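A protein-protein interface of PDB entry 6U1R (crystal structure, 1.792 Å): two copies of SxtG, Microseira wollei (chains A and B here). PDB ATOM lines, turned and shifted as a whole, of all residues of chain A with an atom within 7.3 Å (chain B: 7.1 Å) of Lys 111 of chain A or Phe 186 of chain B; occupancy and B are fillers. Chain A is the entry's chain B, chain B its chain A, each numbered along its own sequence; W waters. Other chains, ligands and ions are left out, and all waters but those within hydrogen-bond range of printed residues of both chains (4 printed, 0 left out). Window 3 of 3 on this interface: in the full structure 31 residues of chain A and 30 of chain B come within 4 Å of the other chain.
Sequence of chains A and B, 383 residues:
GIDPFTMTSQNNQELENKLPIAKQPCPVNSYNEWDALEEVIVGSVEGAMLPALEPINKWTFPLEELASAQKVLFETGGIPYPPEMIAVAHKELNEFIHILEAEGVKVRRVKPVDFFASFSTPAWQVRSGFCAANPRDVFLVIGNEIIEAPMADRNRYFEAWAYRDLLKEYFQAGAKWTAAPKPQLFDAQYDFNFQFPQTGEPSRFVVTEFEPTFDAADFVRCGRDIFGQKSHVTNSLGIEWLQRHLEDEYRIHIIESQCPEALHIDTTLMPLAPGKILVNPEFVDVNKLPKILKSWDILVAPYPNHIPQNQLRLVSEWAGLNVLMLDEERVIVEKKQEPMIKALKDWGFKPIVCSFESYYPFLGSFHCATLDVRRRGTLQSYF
O of Phe 210 of chain B sits at hydrogen-bond distance from NZ of Lys 168 of chain A, 2.9 Å away.
The side-chain hydroxyl of Thr 121 of chain B lies close to the backbone NH of Ala 123 of chain B (3.1 Å). The side-chain hydroxyl of Thr 208 of chain B is in hydrogen-bond range of the backbone NH of Phe 210 of chain B. The side-chain amide oxygen (OE1) of Gln 189 of chain B lies within hydrogen-bond range of the backbone NH (N) of Glu 211 of chain B, 3.1 Å away. The indole nitrogen (NE1) of Trp 124 of chain B sits at hydrogen-bond distance from the backbone carbonyl oxygen (O) of Gln 184 of chain B. The side-chain hydroxyl of Thr 121 of chain B lies within hydrogen-bond range of the backbone NH of Trp 124 of chain B (3.2 Å).
Among the printed residues, pairs that only touch across the chains: Trp 161 of chain A with Gln 184 of chain B, Trp 161 of chain A with Thr 121 of chain B, Trp 161 of chain A with Phe 186 of chain B, Trp 161 of chain A with Pro 122 of chain B, Arg 164 of chain A with Gln 184 of chain B, Trp 161 of chain A with Ala 123 of chain B, Lys 168 of chain A with Glu 211 of chain B and Lys 111 of chain A with Phe 186 of chain B.
Lys 111 of chain A touches one residue of chain B. Printed residues of chain A within 4 Å of Pro 122 of chain B: Trp 161 (3.6 Å). Of the printed residues of chain A, Ala 123 of chain B touches Trp 161. Phe 186 of chain B touches two residues of chain A. The nearest residue of chain B that does not touch Lys 111 of chain A is Gln 184 of chain B (5.1 Å). The nearest residue of chain A that does not touch Phe 186 of chain B is Val 113 of chain A (6.4 Å). The nearest printed residue of chain A that does not touch Pro 122 of chain B is Asp 114 of chain A (4.3 Å).
Printed residues of chain B that touch a printed residue of chain A: Thr 121, Pro 122, Ala 123, Gln 184, Phe 186, Phe 210 and Glu 211. Hydrophobic or aromatic side chains of chain B that line the printed part of chain A: Pro 122, Ala 123, Phe 186 and Phe 210. Hydrophobic or aromatic side chains of chain A that line the printed part of chain B: Trp 161. Among the printed residues, no Asp or Glu carboxylate lies within 4 Å of a Lys or Arg side-chain nitrogen of the other chain.
No position is printed for both chains. Of the 9 pairs that touch across the chains among the printed residues, none has its exchanged pair printed and touching as well.
Water W2 lies within hydrogen-bond range of OE1 of Gln 184 of chain B (2.7 Å), NZ of Lys 111 of chain A (3.0 Å) and OD1 of Asp 165 of chain A (3.3 Å). Water W1 lies within hydrogen-bond range of OE1 of Glu 211 of chain B (2.8 Å) and NH1 of Arg 164 of chain A (2.9 Å). Water W4 lies within hydrogen-bond range of NE2 of Gln 184 of chain B (2.9 Å), NZ of Lys 111 of chain A (2.9 Å) and O of Trp 161 of chain A (3.0 Å).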
ATOM      1  N   SER A  44       7.212   7.669   7.235  1.00  0.00           N
ATOM      2  CA  SER A  44       5.912   7.986   6.656  1.00  0.00           C
ATOM      3  C   SER A  44       6.125   8.637   5.295  1.00  0.00           C
ATOM      4  O   SER A  44       7.051   9.439   5.124  1.00  0.00           O
ATOM      5  CB  SER A  44       5.102   8.935   7.553  1.00  0.00           C
ATOM      6  OG  SER A  44       4.047   9.535   6.816  1.00  0.00           O
ATOM      7  N   GLU A  46       3.412  10.216   3.799  1.00  0.00           N
ATOM      8  CA  GLU A  46       2.357  11.210   3.655  1.00  0.00           C
ATOM      9  C   GLU A  46       2.947  12.606   3.506  1.00  0.00           C
ATOM     10  O   GLU A  46       3.881  12.981   4.224  1.00  0.00           O
ATOM     11  CB  GLU A  46       1.420  11.133   4.857  1.00  0.00           C
ATOM     12  CG  GLU A  46       0.690   9.786   4.912  1.00  0.00           C
ATOM     13  CD  GLU A  46      -0.373   9.729   5.978  1.00  0.00           C
ATOM     14  OE1 GLU A  46      -1.238  10.632   6.008  1.00  0.00           O
ATOM     15  OE2 GLU A  46      -0.336   8.783   6.788  1.00  0.00           O
ATOM     16  N   ARG A 109       4.890   5.645  15.033  1.00  0.00           N
ATOM     17  CA  ARG A 109       4.646   6.425  13.824  1.00  0.00           C
ATOM     18  C   ARG A 109       4.888   7.907  14.087  1.00  0.00           C
ATOM     19  O   ARG A 109       4.696   8.399  15.205  1.00  0.00           O
ATOM     20  CB  ARG A 109       3.221   6.194  13.324  1.00  0.00           C
ATOM     21  CG  ARG A 109       2.992   4.745  12.891  1.00  0.00           C
ATOM     22  CD  ARG A 109       1.519   4.406  12.903  1.00  0.00           C
ATOM     23  NE  ARG A 109       1.199   3.040  12.472  1.00  0.00           N
ATOM     24  CZ  ARG A 109       0.992   2.673  11.210  1.00  0.00           C
ATOM     25  NH1 ARG A 109       1.117   3.555  10.213  1.00  0.00           N
ATOM     26  NH2 ARG A 109       0.668   1.415  10.946  1.00  0.00           N
ATOM     27  N   VAL A 110       5.339   8.614  13.051  1.00  0.00           N
ATOM     28  CA  VAL A 110       5.719  10.018  13.207  1.00  0.00           C
ATOM     29  C   VAL A 110       4.494  10.911  13.104  1.00  0.00           C
ATOM     30  O   VAL A 110       3.384  10.441  12.839  1.00  0.00           O
ATOM     31  CB  VAL A 110       6.775  10.443  12.168  1.00  0.00           C
ATOM     32  CG1 VAL A 110       7.994   9.555  12.265  1.00  0.00           C
ATOM     33  CG2 VAL A 110       6.193  10.418  10.763  1.00  0.00           C
ATOM     34  N   LYS A 111       4.708  12.214  13.281  1.00  0.00           N
ATOM     35  CA  LYS A 111       3.681  13.241  13.167  1.00  0.00           C
ATOM     36  C   LYS A 111       3.559  13.696  11.713  1.00  0.00           C
ATOM     37  O   LYS A 111       4.581  13.967  11.076  1.00  0.00           O
ATOM     38  CB  LYS A 111       4.035  14.426  14.057  1.00  0.00           C
ATOM     39  CG  LYS A 111       2.936  15.473  14.213  1.00  0.00           C
ATOM     40  CD  LYS A 111       3.008  16.124  15.589  1.00  0.00           C
ATOM     41  CE  LYS A 111       2.484  17.551  15.576  1.00  0.00           C
ATOM     42  NZ  LYS A 111       3.608  18.531  15.609  1.00  0.00           N
ATOM     43  N   PRO A 112       2.351  13.791  11.148  1.00  0.00           N
ATOM     44  CA  PRO A 112       2.206  14.408   9.818  1.00  0.00           C
ATOM     45  C   PRO A 112       2.549  15.888   9.872  1.00  0.00           C
ATOM     46  O   PRO A 112       2.058  16.617  10.738  1.00  0.00           O
ATOM     47  CB  PRO A 112       0.728  14.182   9.478  1.00  0.00           C
ATOM     48  CG  PRO A 112       0.293  13.041  10.367  1.00  0.00           C
ATOM     49  CD  PRO A 112       1.079  13.218  11.628  1.00  0.00           C
ATOM     50  N   VAL A 113       3.404  16.334   8.949  1.00  0.00           N
ATOM     51  CA  VAL A 113       3.869  17.715   8.933  1.00  0.00           C
ATOM     52  C   VAL A 113       3.800  18.264   7.512  1.00  0.00           C
ATOM     53  O   VAL A 113       3.569  17.539   6.547  1.00  0.00           O
ATOM     54  CB  VAL A 113       5.295  17.862   9.502  1.00  0.00           C
ATOM     55  CG1 VAL A 113       5.337  17.334  10.928  1.00  0.00           C
ATOM     56  CG2 VAL A 113       6.309  17.142   8.632  1.00  0.00           C
ATOM     57  N   ASP A 114       4.025  19.576   7.407  1.00  0.00           N
ATOM     58  CA  ASP A 114       3.885  20.313   6.151  1.00  0.00           C
ATOM     59  C   ASP A 114       5.227  20.320   5.428  1.00  0.00           C
ATOM     60  O   ASP A 114       6.006  21.285   5.522  1.00  0.00           O
ATOM     61  CB  ASP A 114       3.424  21.745   6.402  1.00  0.00           C
ATOM     62  CG  ASP A 114       2.006  21.843   6.957  1.00  0.00           C
ATOM     63  OD1 ASP A 114       1.198  20.899   6.792  1.00  0.00           O
ATOM     64  OD2 ASP A 114       1.708  22.912   7.539  1.00  0.00           O
ATOM     65  N   PHE A 115       5.494  19.263   4.653  1.00  0.00           N
ATOM     66  CA  PHE A 115       6.702  19.293   3.842  1.00  0.00           C
ATOM     67  C   PHE A 115       6.584  20.241   2.661  1.00  0.00           C
ATOM     68  O   PHE A 115       7.610  20.614   2.101  1.00  0.00           O
ATOM     69  CB  PHE A 115       7.077  17.888   3.352  1.00  0.00           C
ATOM     70  CG  PHE A 115       7.528  16.997   4.450  1.00  0.00           C
ATOM     71  CD1 PHE A 115       8.794  17.152   5.003  1.00  0.00           C
ATOM     72  CD2 PHE A 115       6.690  16.029   4.964  1.00  0.00           C
ATOM     73  CE1 PHE A 115       9.214  16.359   6.049  1.00  0.00           C
ATOM     74  CE2 PHE A 115       7.101  15.240   6.018  1.00  0.00           C
ATOM     75  CZ  PHE A 115       8.376  15.403   6.557  1.00  0.00           C
ATOM     76  N   ALA A 132       9.347  12.380   5.448  1.00  0.00           N
ATOM     77  CA  ALA A 132       9.778  11.641   6.630  1.00  0.00           C
ATOM     78  C   ALA A 132       9.898  10.138   6.361  1.00  0.00           C
ATOM     79  O   ALA A 132       9.647   9.316   7.248  1.00  0.00           O
ATOM     80  CB  ALA A 132       8.825  11.896   7.794  1.00  0.00           C
ATOM     81  N   TRP A 161      11.472  17.585  12.501  1.00  0.00           N
ATOM     82  CA  TRP A 161      10.240  18.110  13.102  1.00  0.00           C
ATOM     83  C   TRP A 161       9.159  17.041  13.239  1.00  0.00           C
ATOM     84  O   TRP A 161       8.389  17.046  14.213  1.00  0.00           O
ATOM     85  CB  TRP A 161       9.723  19.302  12.285  1.00  0.00           C
ATOM     86  CG  TRP A 161      10.412  20.593  12.659  1.00  0.00           C
ATOM     87  CD1 TRP A 161      11.603  20.717  13.288  1.00  0.00           C
ATOM     88  CD2 TRP A 161       9.919  21.922  12.456  1.00  0.00           C
ATOM     89  NE1 TRP A 161      11.890  22.045  13.510  1.00  0.00           N
ATOM     90  CE2 TRP A 161      10.873  22.806  13.004  1.00  0.00           C
ATOM     91  CE3 TRP A 161       8.752  22.450  11.881  1.00  0.00           C
ATOM     92  CZ2 TRP A 161      10.711  24.195  12.986  1.00  0.00           C
ATOM     93  CZ3 TRP A 161       8.587  23.824  11.857  1.00  0.00           C
ATOM     94  CH2 TRP A 161       9.562  24.688  12.409  1.00  0.00           C
ATOM     95  N   ALA A 162       9.073  16.119  12.283  1.00  0.00           N
ATOM     96  CA  ALA A 162       8.055  15.074  12.374  1.00  0.00           C
ATOM     97  C   ALA A 162       8.290  14.119  13.538  1.00  0.00           C
ATOM     98  O   ALA A 162       7.362  13.411  13.940  1.00  0.00           O
ATOM     99  CB  ALA A 162       7.999  14.298  11.055  1.00  0.00           C
ATOM    100  N   TYR A 163       9.496  14.095  14.096  1.00  0.00           N
ATOM    101  CA  TYR A 163       9.875  13.164  15.147  1.00  0.00           C
ATOM    102  C   TYR A 163       9.858  13.799  16.531  1.00  0.00           C
ATOM    103  O   TYR A 163      10.106  13.113  17.517  1.00  0.00           O
ATOM    104  CB  TYR A 163      11.279  12.611  14.850  1.00  0.00           C
ATOM    105  CG  TYR A 163      11.387  11.932  13.504  1.00  0.00           C
ATOM    106  CD1 TYR A 163      11.646  12.664  12.354  1.00  0.00           C
ATOM    107  CD2 TYR A 163      11.218  10.566  13.382  1.00  0.00           C
ATOM    108  CE1 TYR A 163      11.724  12.046  11.102  1.00  0.00           C
ATOM    109  CE2 TYR A 163      11.309   9.943  12.159  1.00  0.00           C
ATOM    110  CZ  TYR A 163      11.565  10.689  11.018  1.00  0.00           C
ATOM    111  OH  TYR A 163      11.658  10.064   9.809  1.00  0.00           O
ATOM    112  N   ARG A 164       9.595  15.098  16.635  1.00  0.00           N
ATOM    113  CA  ARG A 164       9.872  15.773  17.893  1.00  0.00           C
ATOM    114  C   ARG A 164       8.941  15.328  19.018  1.00  0.00           C
ATOM    115  O   ARG A 164       9.353  15.333  20.177  1.00  0.00           O
ATOM    116  CB  ARG A 164       9.828  17.287  17.693  1.00  0.00           C
ATOM    117  CG  ARG A 164      11.137  17.832  17.074  1.00  0.00           C
ATOM    118  CD  ARG A 164      12.348  17.685  18.030  1.00  0.00           C
ATOM    119  NE  ARG A 164      13.632  18.090  17.418  1.00  0.00           N
ATOM    120  CZ  ARG A 164      14.055  19.352  17.398  1.00  0.00           C
ATOM    121  NH1 ARG A 164      13.282  20.311  17.896  1.00  0.00           N
ATOM    122  NH2 ARG A 164      15.219  19.675  16.847  1.00  0.00           N
ATOM    123  N   ASP A 165       7.697  14.944  18.731  1.00  0.00           N
ATOM    124  CA  ASP A 165       6.865  14.431  19.828  1.00  0.00           C
ATOM    125  C   ASP A 165       7.474  13.162  20.436  1.00  0.00           C
ATOM    126  O   ASP A 165       7.517  13.002  21.673  1.00  0.00           O
ATOM    127  CB  ASP A 165       5.439  14.163  19.349  1.00  0.00           C
ATOM    128  CG  ASP A 165       4.629  15.444  19.163  1.00  0.00           C
ATOM    129  OD1 ASP A 165       5.073  16.521  19.622  1.00  0.00           O
ATOM    130  OD2 ASP A 165       3.548  15.371  18.546  1.00  0.00           O
ATOM    131  N   LEU A 166       7.946  12.249  19.585  1.00  0.00           N
ATOM    132  CA  LEU A 166       8.597  11.039  20.080  1.00  0.00           C
ATOM    133  C   LEU A 166       9.888  11.364  20.817  1.00  0.00           C
ATOM    134  O   LEU A 166      10.178  10.768  21.867  1.00  0.00           O
ATOM    135  CB  LEU A 166       8.868  10.060  18.931  1.00  0.00           C
ATOM    136  CG  LEU A 166       7.627   9.328  18.380  1.00  0.00           C
ATOM    137  CD1 LEU A 166       7.878   8.731  17.004  1.00  0.00           C
ATOM    138  CD2 LEU A 166       7.165   8.254  19.359  1.00  0.00           C
ATOM    139  N   LYS A 168      10.731  14.039  22.454  1.00  0.00           N
ATOM    140  CA  LYS A 168      10.427  14.596  23.767  1.00  0.00           C
ATOM    141  C   LYS A 168       9.902  13.526  24.715  1.00  0.00           C
ATOM    142  O   LYS A 168      10.222  13.560  25.911  1.00  0.00           O
ATOM    143  CB  LYS A 168       9.454  15.770  23.631  1.00  0.00           C
ATOM    144  CG  LYS A 168      10.119  16.984  22.989  1.00  0.00           C
ATOM    145  CD  LYS A 168       9.226  18.225  22.908  1.00  0.00           C
ATOM    146  CE  LYS A 168       8.052  18.026  21.979  1.00  0.00           C
ATOM    147  NZ  LYS A 168       7.296  19.328  21.763  1.00  0.00           N
ATOM    148  N   THR B 121      10.727  29.383   9.011  1.00  0.00           N
ATOM    149  CA  THR B 121      10.627  27.946   9.172  1.00  0.00           C
ATOM    150  C   THR B 121       9.316  27.495   8.535  1.00  0.00           C
ATOM    151  O   THR B 121       8.507  28.329   8.086  1.00  0.00           O
ATOM    152  CB  THR B 121      10.638  27.545  10.651  1.00  0.00           C
ATOM    153  OG1 THR B 121       9.377  27.894  11.245  1.00  0.00           O
ATOM    154  CG2 THR B 121      11.748  28.257  11.420  1.00  0.00           C
ATOM    155  N   PRO B 122       9.043  26.195   8.514  1.00  0.00           N
ATOM    156  CA  PRO B 122       7.755  25.733   7.974  1.00  0.00           C
ATOM    157  C   PRO B 122       6.555  26.249   8.752  1.00  0.00           C
ATOM    158  O   PRO B 122       5.436  26.215   8.229  1.00  0.00           O
ATOM    159  CB  PRO B 122       7.876  24.202   8.048  1.00  0.00           C
ATOM    160  CG  PRO B 122       9.374  23.958   7.904  1.00  0.00           C
ATOM    161  CD  PRO B 122       9.983  25.087   8.732  1.00  0.00           C
ATOM    162  N   ALA B 123       6.751  26.756   9.976  1.00  0.00           N
ATOM    163  CA  ALA B 123       5.646  27.149  10.840  1.00  0.00           C
ATOM    164  C   ALA B 123       5.543  28.647  11.126  1.00  0.00           C
ATOM    165  O   ALA B 123       4.493  29.089  11.599  1.00  0.00           O
ATOM    166  CB  ALA B 123       5.753  26.418  12.187  1.00  0.00           C
ATOM    167  N   TRP B 124       6.597  29.430  10.897  1.00  0.00           N
ATOM    168  CA  TRP B 124       6.582  30.840  11.278  1.00  0.00           C
ATOM    169  C   TRP B 124       7.686  31.571  10.533  1.00  0.00           C
ATOM    170  O   TRP B 124       8.604  30.956   9.988  1.00  0.00           O
ATOM    171  CB  TRP B 124       6.739  31.040  12.798  1.00  0.00           C
ATOM    172  CG  TRP B 124       7.913  30.324  13.430  1.00  0.00           C
ATOM    173  CD1 TRP B 124       7.874  29.139  14.089  1.00  0.00           C
ATOM    174  CD2 TRP B 124       9.283  30.772  13.488  1.00  0.00           C
ATOM    175  NE1 TRP B 124       9.131  28.804  14.547  1.00  0.00           N
ATOM    176  CE2 TRP B 124      10.014  29.789  14.193  1.00  0.00           C
ATOM    177  CE3 TRP B 124       9.959  31.896  13.011  1.00  0.00           C
ATOM    178  CZ2 TRP B 124      11.380  29.902  14.435  1.00  0.00           C
ATOM    179  CZ3 TRP B 124      11.307  32.008  13.236  1.00  0.00           C
ATOM    180  CH2 TRP B 124      12.012  31.014  13.957  1.00  0.00           C
ATOM    181  N   ARG B 154      12.448  33.551  18.686  1.00  0.00           N
ATOM    182  CA  ARG B 154      12.498  33.256  17.260  1.00  0.00           C
ATOM    183  C   ARG B 154      13.471  34.150  16.502  1.00  0.00           C
ATOM    184  O   ARG B 154      14.141  33.689  15.584  1.00  0.00           O
ATOM    185  CB  ARG B 154      11.096  33.401  16.656  1.00  0.00           C
ATOM    186  CG  ARG B 154      10.109  32.335  17.087  1.00  0.00           C
ATOM    187  CD  ARG B 154       8.703  32.770  16.700  1.00  0.00           C
ATOM    188  NE  ARG B 154       7.721  31.706  16.895  1.00  0.00           N
ATOM    189  CZ  ARG B 154       6.412  31.912  17.001  1.00  0.00           C
ATOM    190  NH1 ARG B 154       5.919  33.159  16.942  1.00  0.00           N
ATOM    191  NH2 ARG B 154       5.593  30.875  17.151  1.00  0.00           N
ATOM    192  N   PRO B 183      14.963  24.261  18.828  1.00  0.00           N
ATOM    193  CA  PRO B 183      13.523  24.173  19.108  1.00  0.00           C
ATOM    194  C   PRO B 183      12.691  24.562  17.897  1.00  0.00           C
ATOM    195  O   PRO B 183      13.126  25.302  17.014  1.00  0.00           O
ATOM    196  CB  PRO B 183      13.323  25.154  20.273  1.00  0.00           C
ATOM    197  CG  PRO B 183      14.430  26.171  20.103  1.00  0.00           C
ATOM    198  CD  PRO B 183      15.604  25.340  19.609  1.00  0.00           C
ATOM    199  N   GLN B 184      11.456  24.051  17.885  1.00  0.00           N
ATOM    200  CA  GLN B 184      10.500  24.342  16.823  1.00  0.00           C
ATOM    201  C   GLN B 184       9.920  25.745  16.960  1.00  0.00           C
ATOM    202  O   GLN B 184       9.634  26.401  15.950  1.00  0.00           O
ATOM    203  CB  GLN B 184       9.362  23.311  16.842  1.00  0.00           C
ATOM    204  CG  GLN B 184       9.804  21.880  16.578  1.00  0.00           C
ATOM    205  CD  GLN B 184       8.638  20.906  16.450  1.00  0.00           C
ATOM    206  OE1 GLN B 184       7.962  20.575  17.434  1.00  0.00           O
ATOM    207  NE2 GLN B 184       8.382  20.463  15.237  1.00  0.00           N
ATOM    208  N   LEU B 185       9.695  26.179  18.203  1.00  0.00           N
ATOM    209  CA  LEU B 185       9.162  27.491  18.532  1.00  0.00           C
ATOM    210  C   LEU B 185       7.781  27.697  17.906  1.00  0.00           C
ATOM    211  O   LEU B 185       7.441  28.791  17.451  1.00  0.00           O
ATOM    212  CB  LEU B 185      10.140  28.602  18.138  1.00  0.00           C
ATOM    213  CG  LEU B 185      11.550  28.456  18.748  1.00  0.00           C
ATOM    214  CD1 LEU B 185      12.439  29.684  18.437  1.00  0.00           C
ATOM    215  CD2 LEU B 185      11.461  28.239  20.248  1.00  0.00           C
ATOM    216  N   PHE B 186       6.969  26.639  17.939  1.00  0.00           N
ATOM    217  CA  PHE B 186       5.547  26.771  17.659  1.00  0.00           C
ATOM    218  C   PHE B 186       4.877  27.711  18.664  1.00  0.00           C
ATOM    219  O   PHE B 186       5.379  27.974  19.766  1.00  0.00           O
ATOM    220  CB  PHE B 186       4.852  25.400  17.731  1.00  0.00           C
ATOM    221  CG  PHE B 186       5.220  24.430  16.634  1.00  0.00           C
ATOM    222  CD1 PHE B 186       6.056  24.774  15.577  1.00  0.00           C
ATOM    223  CD2 PHE B 186       4.698  23.144  16.664  1.00  0.00           C
ATOM    224  CE1 PHE B 186       6.353  23.853  14.574  1.00  0.00           C
ATOM    225  CE2 PHE B 186       4.987  22.234  15.664  1.00  0.00           C
ATOM    226  CZ  PHE B 186       5.807  22.588  14.621  1.00  0.00           C
ATOM    227  N   ASP B 187       3.677  28.174  18.298  1.00  0.00           N
ATOM    228  CA  ASP B 187       2.904  28.984  19.229  1.00  0.00           C
ATOM    229  C   ASP B 187       2.722  28.292  20.577  1.00  0.00           C
ATOM    230  O   ASP B 187       2.619  28.969  21.600  1.00  0.00           O
ATOM    231  CB  ASP B 187       1.531  29.320  18.635  1.00  0.00           C
ATOM    232  CG  ASP B 187       1.586  30.404  17.572  1.00  0.00           C
ATOM    233  OD1 ASP B 187       2.648  31.034  17.356  1.00  0.00           O
ATOM    234  OD2 ASP B 187       0.522  30.643  16.956  1.00  0.00           O
ATOM    235  N   ALA B 188       2.686  26.951  20.602  1.00  0.00           N
ATOM    236  CA  ALA B 188       2.485  26.225  21.856  1.00  0.00           C
ATOM    237  C   ALA B 188       3.585  26.476  22.896  1.00  0.00           C
ATOM    238  O   ALA B 188       3.384  26.163  24.074  1.00  0.00           O
ATOM    239  CB  ALA B 188       2.383  24.723  21.589  1.00  0.00           C
ATOM    240  N   GLN B 189       4.740  27.003  22.484  1.00  0.00           N
ATOM    241  CA  GLN B 189       5.837  27.316  23.399  1.00  0.00           C
ATOM    242  C   GLN B 189       5.581  28.586  24.209  1.00  0.00           C
ATOM    243  O   GLN B 189       6.336  28.874  25.141  1.00  0.00           O
ATOM    244  CB  GLN B 189       7.144  27.429  22.591  1.00  0.00           C
ATOM    245  CG  GLN B 189       8.423  27.673  23.430  1.00  0.00           C
ATOM    246  CD  GLN B 189       8.715  26.573  24.438  1.00  0.00           C
ATOM    247  OE1 GLN B 189       8.149  25.488  24.374  1.00  0.00           O
ATOM    248  NE2 GLN B 189       9.618  26.862  25.390  1.00  0.00           N
ATOM    249  N   TYR B 190       4.507  29.333  23.915  1.00  0.00           N
ATOM    250  CA  TYR B 190       4.262  30.618  24.551  1.00  0.00           C
ATOM    251  C   TYR B 190       2.830  30.673  25.077  1.00  0.00           C
ATOM    252  O   TYR B 190       1.903  30.183  24.428  1.00  0.00           O
ATOM    253  CB  TYR B 190       4.507  31.776  23.563  1.00  0.00           C
ATOM    254  CG  TYR B 190       5.769  31.622  22.747  1.00  0.00           C
ATOM    255  CD1 TYR B 190       7.011  31.863  23.307  1.00  0.00           C
ATOM    256  CD2 TYR B 190       5.712  31.223  21.418  1.00  0.00           C
ATOM    257  CE1 TYR B 190       8.190  31.710  22.552  1.00  0.00           C
ATOM    258  CE2 TYR B 190       6.861  31.070  20.657  1.00  0.00           C
ATOM    259  CZ  TYR B 190       8.102  31.316  21.232  1.00  0.00           C
ATOM    260  OH  TYR B 190       9.229  31.145  20.455  1.00  0.00           O
ATOM    261  N   PHE B 192      -0.155  32.666  25.438  1.00  0.00           N
ATOM    262  CA  PHE B 192      -0.723  33.899  24.904  1.00  0.00           C
ATOM    263  C   PHE B 192      -1.789  34.503  25.808  1.00  0.00           C
ATOM    264  O   PHE B 192      -2.295  35.583  25.498  1.00  0.00           O
ATOM    265  CB  PHE B 192      -1.270  33.650  23.496  1.00  0.00           C
ATOM    266  CG  PHE B 192      -0.189  33.492  22.464  1.00  0.00           C
ATOM    267  CD1 PHE B 192       0.401  34.609  21.888  1.00  0.00           C
ATOM    268  CD2 PHE B 192       0.277  32.234  22.104  1.00  0.00           C
ATOM    269  CE1 PHE B 192       1.414  34.476  20.946  1.00  0.00           C
ATOM    270  CE2 PHE B 192       1.288  32.088  21.156  1.00  0.00           C
ATOM    271  CZ  PHE B 192       1.857  33.209  20.576  1.00  0.00           C
ATOM    272  N   THR B 208       6.140  28.160  28.020  1.00  0.00           N
ATOM    273  CA  THR B 208       5.427  26.986  28.497  1.00  0.00           C
ATOM    274  C   THR B 208       6.415  25.837  28.650  1.00  0.00           C
ATOM    275  O   THR B 208       7.641  26.033  28.595  1.00  0.00           O
ATOM    276  CB  THR B 208       4.318  26.592  27.520  1.00  0.00           C
ATOM    277  OG1 THR B 208       4.925  26.109  26.311  1.00  0.00           O
ATOM    278  CG2 THR B 208       3.417  27.770  27.202  1.00  0.00           C
ATOM    279  N   PHE B 210       6.270  23.196  26.454  1.00  0.00           N
ATOM    280  CA  PHE B 210       6.102  22.461  25.205  1.00  0.00           C
ATOM    281  C   PHE B 210       7.406  21.780  24.765  1.00  0.00           C
ATOM    282  O   PHE B 210       7.391  20.613  24.353  1.00  0.00           O
ATOM    283  CB  PHE B 210       5.561  23.431  24.155  1.00  0.00           C
ATOM    284  CG  PHE B 210       5.647  22.943  22.745  1.00  0.00           C
ATOM    285  CD1 PHE B 210       4.772  21.975  22.273  1.00  0.00           C
ATOM    286  CD2 PHE B 210       6.575  23.488  21.877  1.00  0.00           C
ATOM    287  CE1 PHE B 210       4.842  21.545  20.964  1.00  0.00           C
ATOM    288  CE2 PHE B 210       6.658  23.061  20.579  1.00  0.00           C
ATOM    289  CZ  PHE B 210       5.784  22.085  20.113  1.00  0.00           C
ATOM    290  N   GLU B 211       8.535  22.481  24.836  1.00  0.00           N
ATOM    291  CA  GLU B 211       9.807  21.922  24.397  1.00  0.00           C
ATOM    292  C   GLU B 211      10.947  22.591  25.154  1.00  0.00           C
ATOM    293  O   GLU B 211      10.768  23.665  25.733  1.00  0.00           O
ATOM    294  CB  GLU B 211       9.999  22.097  22.888  1.00  0.00           C
ATOM    295  CG  GLU B 211      10.284  23.526  22.499  1.00  0.00           C
ATOM    296  CD  GLU B 211      10.200  23.738  21.008  1.00  0.00           C
ATOM    297  OE1 GLU B 211      10.522  22.803  20.229  1.00  0.00           O
ATOM    298  OE2 GLU B 211       9.797  24.854  20.638  1.00  0.00           O
HETATM  299  O   HOH W   1      12.555  20.866  20.696  1.00  0.00           O
HETATM  300  O   HOH W   2       5.743  19.051  17.618  1.00  0.00           O
HETATM  301  O   HOH W   3       9.036  20.464  19.935  1.00  0.00           O
HETATM  302  O   HOH W   4       6.150  18.973  14.232  1.00  0.00           O
